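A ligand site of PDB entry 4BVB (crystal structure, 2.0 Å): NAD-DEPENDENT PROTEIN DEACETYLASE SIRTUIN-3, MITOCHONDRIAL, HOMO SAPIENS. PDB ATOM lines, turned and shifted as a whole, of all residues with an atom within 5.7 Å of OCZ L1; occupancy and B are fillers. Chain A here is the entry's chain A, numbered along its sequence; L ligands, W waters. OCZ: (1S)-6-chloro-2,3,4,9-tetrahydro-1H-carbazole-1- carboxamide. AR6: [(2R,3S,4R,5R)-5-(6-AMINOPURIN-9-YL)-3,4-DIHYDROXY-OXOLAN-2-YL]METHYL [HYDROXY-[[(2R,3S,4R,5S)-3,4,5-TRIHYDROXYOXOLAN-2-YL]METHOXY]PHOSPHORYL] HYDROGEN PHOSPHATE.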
ATOM      1  N   ALA A  31       3.873  30.095 -10.194  1.00  0.00           N
ATOM      2  CA  ALA A  31       4.254  29.415  -8.931  1.00  0.00           C
ATOM      3  C   ALA A  31       3.115  29.255  -7.948  1.00  0.00           C
ATOM      4  O   ALA A  31       3.123  28.328  -7.054  1.00  0.00           O
ATOM      5  CB  ALA A  31       5.442  30.111  -8.273  1.00  0.00           C
ATOM      6  N   SER A  34       1.467  25.840  -7.370  1.00  0.00           N
ATOM      7  CA  SER A  34       2.196  24.818  -6.632  1.00  0.00           C
ATOM      8  C   SER A  34       2.439  25.129  -5.161  1.00  0.00           C
ATOM      9  O   SER A  34       2.923  24.245  -4.447  1.00  0.00           O
ATOM     10  CB  SER A  34       3.517  24.503  -7.300  1.00  0.00           C
ATOM     11  OG  SER A  34       3.216  23.879  -8.548  1.00  0.00           O
ATOM     12  N   ILE A  39       5.426  23.979  -2.384  1.00  0.00           N
ATOM     13  CA  ILE A  39       6.532  24.684  -3.057  1.00  0.00           C
ATOM     14  C   ILE A  39       6.184  26.182  -2.927  1.00  0.00           C
ATOM     15  O   ILE A  39       5.081  26.601  -3.371  1.00  0.00           O
ATOM     16  CB  ILE A  39       6.638  24.297  -4.548  1.00  0.00           C
ATOM     17  CG1 ILE A  39       6.633  22.760  -4.644  1.00  0.00           C
ATOM     18  CG2 ILE A  39       7.845  24.957  -5.227  1.00  0.00           C
ATOM     19  CD1 ILE A  39       6.974  22.231  -6.014  1.00  0.00           C
ATOM     20  N   PRO A  40       7.085  26.981  -2.334  1.00  0.00           N
ATOM     21  CA  PRO A  40       6.831  28.438  -2.233  1.00  0.00           C
ATOM     22  C   PRO A  40       6.834  29.109  -3.612  1.00  0.00           C
ATOM     23  O   PRO A  40       7.520  28.638  -4.540  1.00  0.00           O
ATOM     24  CB  PRO A  40       8.013  28.970  -1.370  1.00  0.00           C
ATOM     25  CG  PRO A  40       8.722  27.727  -0.823  1.00  0.00           C
ATOM     26  CD  PRO A  40       8.429  26.609  -1.825  1.00  0.00           C
ATOM     27  N   ASP A  41       6.099  30.216  -3.718  1.00  0.00           N
ATOM     28  CA  ASP A  41       6.159  31.093  -4.903  1.00  0.00           C
ATOM     29  C   ASP A  41       7.298  32.090  -4.675  1.00  0.00           C
ATOM     30  O   ASP A  41       8.112  31.904  -3.765  1.00  0.00           O
ATOM     31  CB  ASP A  41       4.785  31.771  -5.126  1.00  0.00           C
ATOM     32  CG  ASP A  41       4.398  32.772  -4.046  1.00  0.00           C
ATOM     33  OD1 ASP A  41       5.202  33.134  -3.095  1.00  0.00           O
ATOM     34  OD2 ASP A  41       3.233  33.164  -4.132  1.00  0.00           O
ATOM     35  N   PHE A  42       7.346  33.154  -5.444  1.00  0.00           N
ATOM     36  CA  PHE A  42       8.434  34.067  -5.270  1.00  0.00           C
ATOM     37  C   PHE A  42       8.109  35.255  -4.426  1.00  0.00           C
ATOM     38  O   PHE A  42       8.956  35.676  -3.583  1.00  0.00           O
ATOM     39  CB  PHE A  42       8.960  34.534  -6.638  1.00  0.00           C
ATOM     40  CG  PHE A  42       9.678  33.480  -7.390  1.00  0.00           C
ATOM     41  CD1 PHE A  42       8.987  32.660  -8.267  1.00  0.00           C
ATOM     42  CD2 PHE A  42      11.065  33.395  -7.326  1.00  0.00           C
ATOM     43  CE1 PHE A  42       9.694  31.663  -9.007  1.00  0.00           C
ATOM     44  CE2 PHE A  42      11.771  32.447  -8.065  1.00  0.00           C
ATOM     45  CZ  PHE A  42      11.049  31.561  -8.891  1.00  0.00           C
ATOM     46  N   LEU A  49       9.864  32.863  -1.813  1.00  0.00           N
ATOM     47  CA  LEU A  49      11.285  32.678  -1.867  1.00  0.00           C
ATOM     48  C   LEU A  49      12.060  33.995  -1.677  1.00  0.00           C
ATOM     49  O   LEU A  49      13.110  33.987  -1.074  1.00  0.00           O
ATOM     50  CB  LEU A  49      11.729  32.030  -3.219  1.00  0.00           C
ATOM     51  CG  LEU A  49      11.235  30.597  -3.445  1.00  0.00           C
ATOM     52  CD1 LEU A  49      11.304  30.175  -4.917  1.00  0.00           C
ATOM     53  CD2 LEU A  49      12.027  29.639  -2.499  1.00  0.00           C
ATOM     54  N   PHE A  65      18.908  32.968  -8.582  1.00  0.00           N
ATOM     55  CA  PHE A  65      18.429  32.513  -9.866  1.00  0.00           C
ATOM     56  C   PHE A  65      19.049  33.273 -11.069  1.00  0.00           C
ATOM     57  O   PHE A  65      18.417  33.335 -12.171  1.00  0.00           O
ATOM     58  CB  PHE A  65      16.916  32.698  -9.883  1.00  0.00           C
ATOM     59  CG  PHE A  65      16.191  32.012  -8.743  1.00  0.00           C
ATOM     60  CD1 PHE A  65      16.190  30.639  -8.622  1.00  0.00           C
ATOM     61  CD2 PHE A  65      15.482  32.747  -7.820  1.00  0.00           C
ATOM     62  CE1 PHE A  65      15.516  30.007  -7.568  1.00  0.00           C
ATOM     63  CE2 PHE A  65      14.801  32.124  -6.775  1.00  0.00           C
ATOM     64  CZ  PHE A  65      14.812  30.747  -6.676  1.00  0.00           C
ATOM     65  N   PHE A  77      22.501  28.221  -5.131  1.00  0.00           N
ATOM     66  CA  PHE A  77      21.508  27.586  -6.036  1.00  0.00           C
ATOM     67  C   PHE A  77      21.299  26.066  -5.803  1.00  0.00           C
ATOM     68  O   PHE A  77      20.157  25.539  -5.797  1.00  0.00           O
ATOM     69  CB  PHE A  77      21.903  27.753  -7.538  1.00  0.00           C
ATOM     70  CG  PHE A  77      20.968  26.990  -8.466  1.00  0.00           C
ATOM     71  CD1 PHE A  77      19.697  27.455  -8.740  1.00  0.00           C
ATOM     72  CD2 PHE A  77      21.308  25.729  -8.918  1.00  0.00           C
ATOM     73  CE1 PHE A  77      18.820  26.702  -9.533  1.00  0.00           C
ATOM     74  CE2 PHE A  77      20.428  24.967  -9.716  1.00  0.00           C
ATOM     75  CZ  PHE A  77      19.194  25.466 -10.009  1.00  0.00           C
ATOM     76  N   LEU A  84      14.001  21.823  -3.649  1.00  0.00           N
ATOM     77  CA  LEU A  84      12.963  21.996  -4.650  1.00  0.00           C
ATOM     78  C   LEU A  84      12.945  20.864  -5.651  1.00  0.00           C
ATOM     79  O   LEU A  84      12.087  20.859  -6.561  1.00  0.00           O
ATOM     80  CB  LEU A  84      13.164  23.360  -5.427  1.00  0.00           C
ATOM     81  CG  LEU A  84      13.068  24.651  -4.631  1.00  0.00           C
ATOM     82  CD1 LEU A  84      13.340  25.945  -5.434  1.00  0.00           C
ATOM     83  CD2 LEU A  84      11.690  24.773  -3.968  1.00  0.00           C
ATOM     84  N   GLN A 113       5.371  28.645 -16.264  1.00  0.00           N
ATOM     85  CA  GLN A 113       6.611  29.196 -15.764  1.00  0.00           C
ATOM     86  C   GLN A 113       7.271  28.360 -14.717  1.00  0.00           C
ATOM     87  O   GLN A 113       8.313  28.764 -14.239  1.00  0.00           O
ATOM     88  CB  GLN A 113       6.316  30.569 -15.177  1.00  0.00           C
ATOM     89  CG  GLN A 113       5.776  31.476 -16.273  1.00  0.00           C
ATOM     90  CD  GLN A 113       5.062  32.698 -15.668  1.00  0.00           C
ATOM     91  OE1 GLN A 113       5.624  33.803 -15.649  1.00  0.00           O
ATOM     92  NE2 GLN A 113       3.848  32.479 -15.123  1.00  0.00           N
ATOM     93  N   ASN A 114       6.653  27.228 -14.319  1.00  0.00           N
ATOM     94  CA  ASN A 114       7.217  26.432 -13.221  1.00  0.00           C
ATOM     95  C   ASN A 114       8.232  25.422 -13.688  1.00  0.00           C
ATOM     96  O   ASN A 114       8.120  24.916 -14.817  1.00  0.00           O
ATOM     97  CB  ASN A 114       6.131  25.699 -12.407  1.00  0.00           C
ATOM     98  CG  ASN A 114       5.154  26.657 -11.725  1.00  0.00           C
ATOM     99  OD1 ASN A 114       5.421  27.873 -11.654  1.00  0.00           O
ATOM    100  ND2 ASN A 114       3.961  26.116 -11.305  1.00  0.00           N
ATOM    101  N   ILE A 115       9.200  25.104 -12.810  1.00  0.00           N
ATOM    102  CA  ILE A 115      10.222  24.095 -13.093  1.00  0.00           C
ATOM    103  C   ILE A 115      10.004  22.803 -12.286  1.00  0.00           C
ATOM    104  O   ILE A 115      10.775  21.844 -12.419  1.00  0.00           O
ATOM    105  CB  ILE A 115      11.613  24.668 -12.873  1.00  0.00           C
ATOM    106  CG1 ILE A 115      11.707  25.165 -11.423  1.00  0.00           C
ATOM    107  CG2 ILE A 115      11.836  25.858 -13.842  1.00  0.00           C
ATOM    108  CD1 ILE A 115      13.131  25.360 -10.964  1.00  0.00           C
ATOM    109  N   ASP A 116       8.929  22.760 -11.504  1.00  0.00           N
ATOM    110  CA  ASP A 116       8.666  21.654 -10.552  1.00  0.00           C
ATOM    111  C   ASP A 116       8.251  20.360 -11.318  1.00  0.00           C
ATOM    112  O   ASP A 116       8.253  19.297 -10.752  1.00  0.00           O
ATOM    113  CB  ASP A 116       7.601  22.070  -9.481  1.00  0.00           C
ATOM    114  CG  ASP A 116       6.256  22.585 -10.070  1.00  0.00           C
ATOM    115  OD1 ASP A 116       5.713  21.984 -11.019  1.00  0.00           O
ATOM    116  OD2 ASP A 116       5.687  23.613  -9.552  1.00  0.00           O
ATOM    117  N   HIS A 133      10.021  28.037 -18.650  1.00  0.00           N
ATOM    118  CA  HIS A 133      11.262  28.269 -17.870  1.00  0.00           C
ATOM    119  C   HIS A 133      12.164  27.046 -17.728  1.00  0.00           C
ATOM    120  O   HIS A 133      13.038  27.006 -16.835  1.00  0.00           O
ATOM    121  CB  HIS A 133      10.967  28.939 -16.500  1.00  0.00           C
ATOM    122  CG  HIS A 133      10.449  30.336 -16.637  1.00  0.00           C
ATOM    123  ND1 HIS A 133       9.887  31.028 -15.603  1.00  0.00           N
ATOM    124  CD2 HIS A 133      10.363  31.142 -17.713  1.00  0.00           C
ATOM    125  CE1 HIS A 133       9.492  32.218 -16.022  1.00  0.00           C
ATOM    126  NE2 HIS A 133       9.774  32.312 -17.304  1.00  0.00           N
ATOM    127  N   ILE A 176      17.267  24.847 -16.516  1.00  0.00           N
ATOM    128  CA  ILE A 176      16.337  25.811 -16.001  1.00  0.00           C
ATOM    129  C   ILE A 176      16.667  27.168 -16.656  1.00  0.00           C
ATOM    130  O   ILE A 176      17.854  27.477 -16.835  1.00  0.00           O
ATOM    131  CB  ILE A 176      16.519  25.956 -14.455  1.00  0.00           C
ATOM    132  CG1 ILE A 176      16.424  24.608 -13.710  1.00  0.00           C
ATOM    133  CG2 ILE A 176      15.451  26.874 -13.921  1.00  0.00           C
ATOM    134  CD1 ILE A 176      15.043  23.978 -13.669  1.00  0.00           C
ATOM    135  N   VAL A 177      15.665  27.983 -16.928  1.00  0.00           N
ATOM    136  CA  VAL A 177      15.934  29.289 -17.498  1.00  0.00           C
ATOM    137  C   VAL A 177      16.178  30.283 -16.374  1.00  0.00           C
ATOM    138  O   VAL A 177      15.224  30.735 -15.689  1.00  0.00           O
ATOM    139  CB  VAL A 177      14.747  29.766 -18.348  1.00  0.00           C
ATOM    140  CG1 VAL A 177      14.996  31.198 -18.851  1.00  0.00           C
ATOM    141  CG2 VAL A 177      14.515  28.765 -19.529  1.00  0.00           C
ATOM    142  N   PHE A 178      17.455  30.578 -16.124  1.00  0.00           N
ATOM    143  CA  PHE A 178      17.745  31.586 -15.096  1.00  0.00           C
ATOM    144  C   PHE A 178      17.216  32.922 -15.538  1.00  0.00           C
ATOM    145  O   PHE A 178      17.032  33.132 -16.755  1.00  0.00           O
ATOM    146  CB  PHE A 178      19.244  31.632 -14.824  1.00  0.00           C
ATOM    147  CG  PHE A 178      19.703  30.600 -13.879  1.00  0.00           C
ATOM    148  CD1 PHE A 178      18.960  29.430 -13.716  1.00  0.00           C
ATOM    149  CD2 PHE A 178      20.868  30.763 -13.163  1.00  0.00           C
ATOM    150  CE1 PHE A 178      19.383  28.437 -12.796  1.00  0.00           C
ATOM    151  CE2 PHE A 178      21.280  29.794 -12.257  1.00  0.00           C
ATOM    152  CZ  PHE A 178      20.562  28.606 -12.097  1.00  0.00           C
ATOM    153  N   PHE A 179      17.000  33.815 -14.566  1.00  0.00           N
ATOM    154  CA  PHE A 179      16.310  35.096 -14.770  1.00  0.00           C
ATOM    155  C   PHE A 179      17.010  35.888 -15.867  1.00  0.00           C
ATOM    156  O   PHE A 179      18.217  36.082 -15.798  1.00  0.00           O
ATOM    157  CB  PHE A 179      16.285  35.911 -13.486  1.00  0.00           C
ATOM    158  CG  PHE A 179      15.353  35.392 -12.425  1.00  0.00           C
ATOM    159  CD1 PHE A 179      14.742  34.098 -12.525  1.00  0.00           C
ATOM    160  CD2 PHE A 179      15.099  36.174 -11.276  1.00  0.00           C
ATOM    161  CE1 PHE A 179      13.876  33.646 -11.540  1.00  0.00           C
ATOM    162  CE2 PHE A 179      14.239  35.715 -10.281  1.00  0.00           C
ATOM    163  CZ  PHE A 179      13.615  34.457 -10.436  1.00  0.00           C
HETATM  164  NAQ OCZ L   1       7.039  26.076  -8.668  1.00  0.00           N
HETATM  165  OAP OCZ L   1       8.554  25.727 -10.281  1.00  0.00           O
HETATM  166  CAO OCZ L   1       8.073  26.456  -9.403  1.00  0.00           C
HETATM  167  NAG OCZ L   1       9.773  28.611 -11.265  1.00  0.00           N
HETATM  168  CAJ OCZ L   1      11.475  27.835  -8.111  1.00  0.00           C
HETATM  169  CAD OCZ L   1      11.592  29.284 -12.763  1.00  0.00           C
HETATM  170  CAC OCZ L   1      12.934  29.557 -12.894  1.00  0.00           C
HETATM  171  CAE OCZ L   1      11.062  28.903 -11.583  1.00  0.00           C
HETATM  172 CL   OCZ L   1      15.551  29.688 -11.990  1.00  0.00          CL
HETATM  173  CAF OCZ L   1      11.863  28.636 -10.522  1.00  0.00           C
HETATM  174  CAA OCZ L   1      13.197  28.876 -10.590  1.00  0.00           C
HETATM  175  CAH OCZ L   1      11.095  28.168  -9.506  1.00  0.00           C
HETATM  176  CAI OCZ L   1       9.780  28.165  -9.969  1.00  0.00           C
HETATM  177  CAB OCZ L   1      13.774  29.340 -11.797  1.00  0.00           C
HETATM  178  CAM OCZ L   1      10.200  27.253  -7.277  1.00  0.00           C
HETATM  179  CAK OCZ L   1       8.626  27.801  -9.146  1.00  0.00           C
HETATM  180  CAL OCZ L   1       8.972  28.083  -7.604  1.00  0.00           C
HETATM  181  N1  AR6 L   2      -3.951  30.786  -4.263  1.00  0.00           N
HETATM  182  C2  AR6 L   2      -4.128  31.842  -5.108  1.00  0.00           C
HETATM  183  N3  AR6 L   2      -3.091  32.553  -5.559  1.00  0.00           N
HETATM  184  C4  AR6 L   2      -1.835  32.267  -5.146  1.00  0.00           C
HETATM  185  C5  AR6 L   2      -1.609  31.192  -4.194  1.00  0.00           C
HETATM  186  C6  AR6 L   2      -2.757  30.440  -3.771  1.00  0.00           C
HETATM  187  N6  AR6 L   2      -2.629  29.399  -2.921  1.00  0.00           N
HETATM  188  N7  AR6 L   2      -0.263  31.155  -3.912  1.00  0.00           N
HETATM  189  C8  AR6 L   2       0.296  32.154  -4.652  1.00  0.00           C
HETATM  190  N9  AR6 L   2      -0.631  32.829  -5.336  1.00  0.00           N
HETATM  191  PA  AR6 L   2       5.001  34.931  -8.364  1.00  0.00           P
HETATM  192  PB  AR6 L   2       5.265  33.590 -10.941  1.00  0.00           P
HETATM  193  C1' AR6 L   2      -0.390  33.913  -6.259  1.00  0.00           C
HETATM  194  O1A AR6 L   2       5.425  34.518  -6.984  1.00  0.00           O
HETATM  195  O1B AR6 L   2       5.319  32.126 -11.283  1.00  0.00           O
HETATM  196  C1D AR6 L   2      10.647  34.386 -11.646  1.00  0.00           C
HETATM  197  O1D AR6 L   2      11.560  35.043 -12.578  1.00  0.00           O
HETATM  198  C2' AR6 L   2       0.430  35.028  -5.640  1.00  0.00           C
HETATM  199  O2' AR6 L   2      -0.584  35.878  -5.043  1.00  0.00           O
HETATM  200  O2A AR6 L   2       5.544  36.166  -9.063  1.00  0.00           O
HETATM  201  O2B AR6 L   2       4.172  34.479 -11.454  1.00  0.00           O
HETATM  202  C2D AR6 L   2      10.625  32.972 -12.134  1.00  0.00           C
HETATM  203  O2D AR6 L   2      11.144  33.017 -13.500  1.00  0.00           O
HETATM  204  C3' AR6 L   2       1.060  35.617  -6.887  1.00  0.00           C
HETATM  205  O3' AR6 L   2       0.072  36.445  -7.526  1.00  0.00           O
HETATM  206  O3A AR6 L   2       5.389  33.688  -9.319  1.00  0.00           O
HETATM  207  C3D AR6 L   2       9.142  32.656 -12.199  1.00  0.00           C
HETATM  208  O3D AR6 L   2       8.760  31.669 -13.186  1.00  0.00           O
HETATM  209  C4' AR6 L   2       1.228  34.398  -7.811  1.00  0.00           C
HETATM  210  O4' AR6 L   2       0.422  33.333  -7.285  1.00  0.00           O
HETATM  211  C4D AR6 L   2       8.489  33.987 -12.472  1.00  0.00           C
HETATM  212  O4D AR6 L   2       9.376  34.953 -11.951  1.00  0.00           O
HETATM  213  C5' AR6 L   2       2.691  33.904  -7.773  1.00  0.00           C
HETATM  214  O5' AR6 L   2       3.437  35.012  -8.273  1.00  0.00           O
HETATM  215  C5D AR6 L   2       7.590  33.906 -11.250  1.00  0.00           C
HETATM  216  O5D AR6 L   2       6.414  34.294 -11.763  1.00  0.00           O
HETATM  217  O   HOH W   1       7.002  30.206 -11.568  1.00  0.00           O
HETATM  218  O   HOH W   2       5.544  27.131  -6.450  1.00  0.00           O
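CG2 of Ile 39 touches NAQ of OCZ L1, at 3.7 Å. Pro 40 touches OCZ L1 (O to CAL, 3.4 Å). CZ of Phe 42 touches CAF of OCZ L1, at 3.4 Å. CD1 of Leu 49 touches CAM of OCZ L1 (3.9 Å). Phe 65 touches OCZ L1. Leu 84 touches OCZ L1 (CD1 to CAJ, 3.8 Å). CB of Asn 114 touches OAP of OCZ L1, at 3.2 Å. ND1 of His 133 touches CAD of OCZ L1 (3.7 Å). Ile 176 touches OCZ L1. O of Val 177 touches CAC of OCZ L1, 3.8 Å away. CD1 of Phe 178 touches CL of OCZ L1, at 3.8 Å.
OD2 of Asp 116 lies within hydrogen-bond range of OG of Ser 34 (2.7 Å). OD1 of Asn 114 sits at hydrogen-bond distance from N of Ala 31, at 3.1 Å. O of Gln 113 lies within hydrogen-bond range of ND1 of His 133, 3.1 Å away. O of Phe 42 lies within hydrogen-bond range of N of Leu 49 (3.4 Å). The backbone carbonyl oxygen (O) of Phe 65 lies within hydrogen-bond range of the backbone NH (N) of Phe 179 (2.8 Å). N of Ile 39 lies within hydrogen-bond range of O of Ser 34 (3.3 Å). The backbone NH (N) of Val 177 lies within hydrogen-bond range of the backbone carbonyl oxygen (O) of His 133 (2.8 Å). The backbone NH of Leu 49 sits at hydrogen-bond distance from the backbone carbonyl oxygen of Asp 41, 2.8 Å away.
Water W1 lies within hydrogen-bond range of an oxygen (O1B) of AR6 L2 (2.6 Å), the side-chain amide oxygen of Asn 114 (2.8 Å), a nitrogen (NAG) of OCZ L1 (3.2 Å), the backbone carbonyl oxygen of Gln 113 (3.3 Å) and the backbone NH of Ala 31 (3.4 Å).
An oxygen (OAP) of OCZ L1 lies within hydrogen-bond range of the backbone NH of Ile 115 (2.7 Å). N of Asp 116 sits at hydrogen-bond distance from OAP of OCZ L1 (3.2 Å). The side-chain carboxylate (OD2) of Asp 116 sits at hydrogen-bond distance from a nitrogen (NAQ) of OCZ L1 (2.9 Å). O of Gln 113 sits at hydrogen-bond distance from NAG of OCZ L1 (3.3 Å). O of Gln 113 sits at hydrogen-bond distance from O3D of AR6 L2 (3.1 Å). The backbone NH of Phe 42 sits at hydrogen-bond distance from an oxygen (O1A) of AR6 L2, at 2.8 Å. ND1 of His 133 lies within hydrogen-bond range of O3D of AR6 L2, 2.7 Å away. O1B of AR6 L2 sits at hydrogen-bond distance from N of Ala 31, at 2.7 Å.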
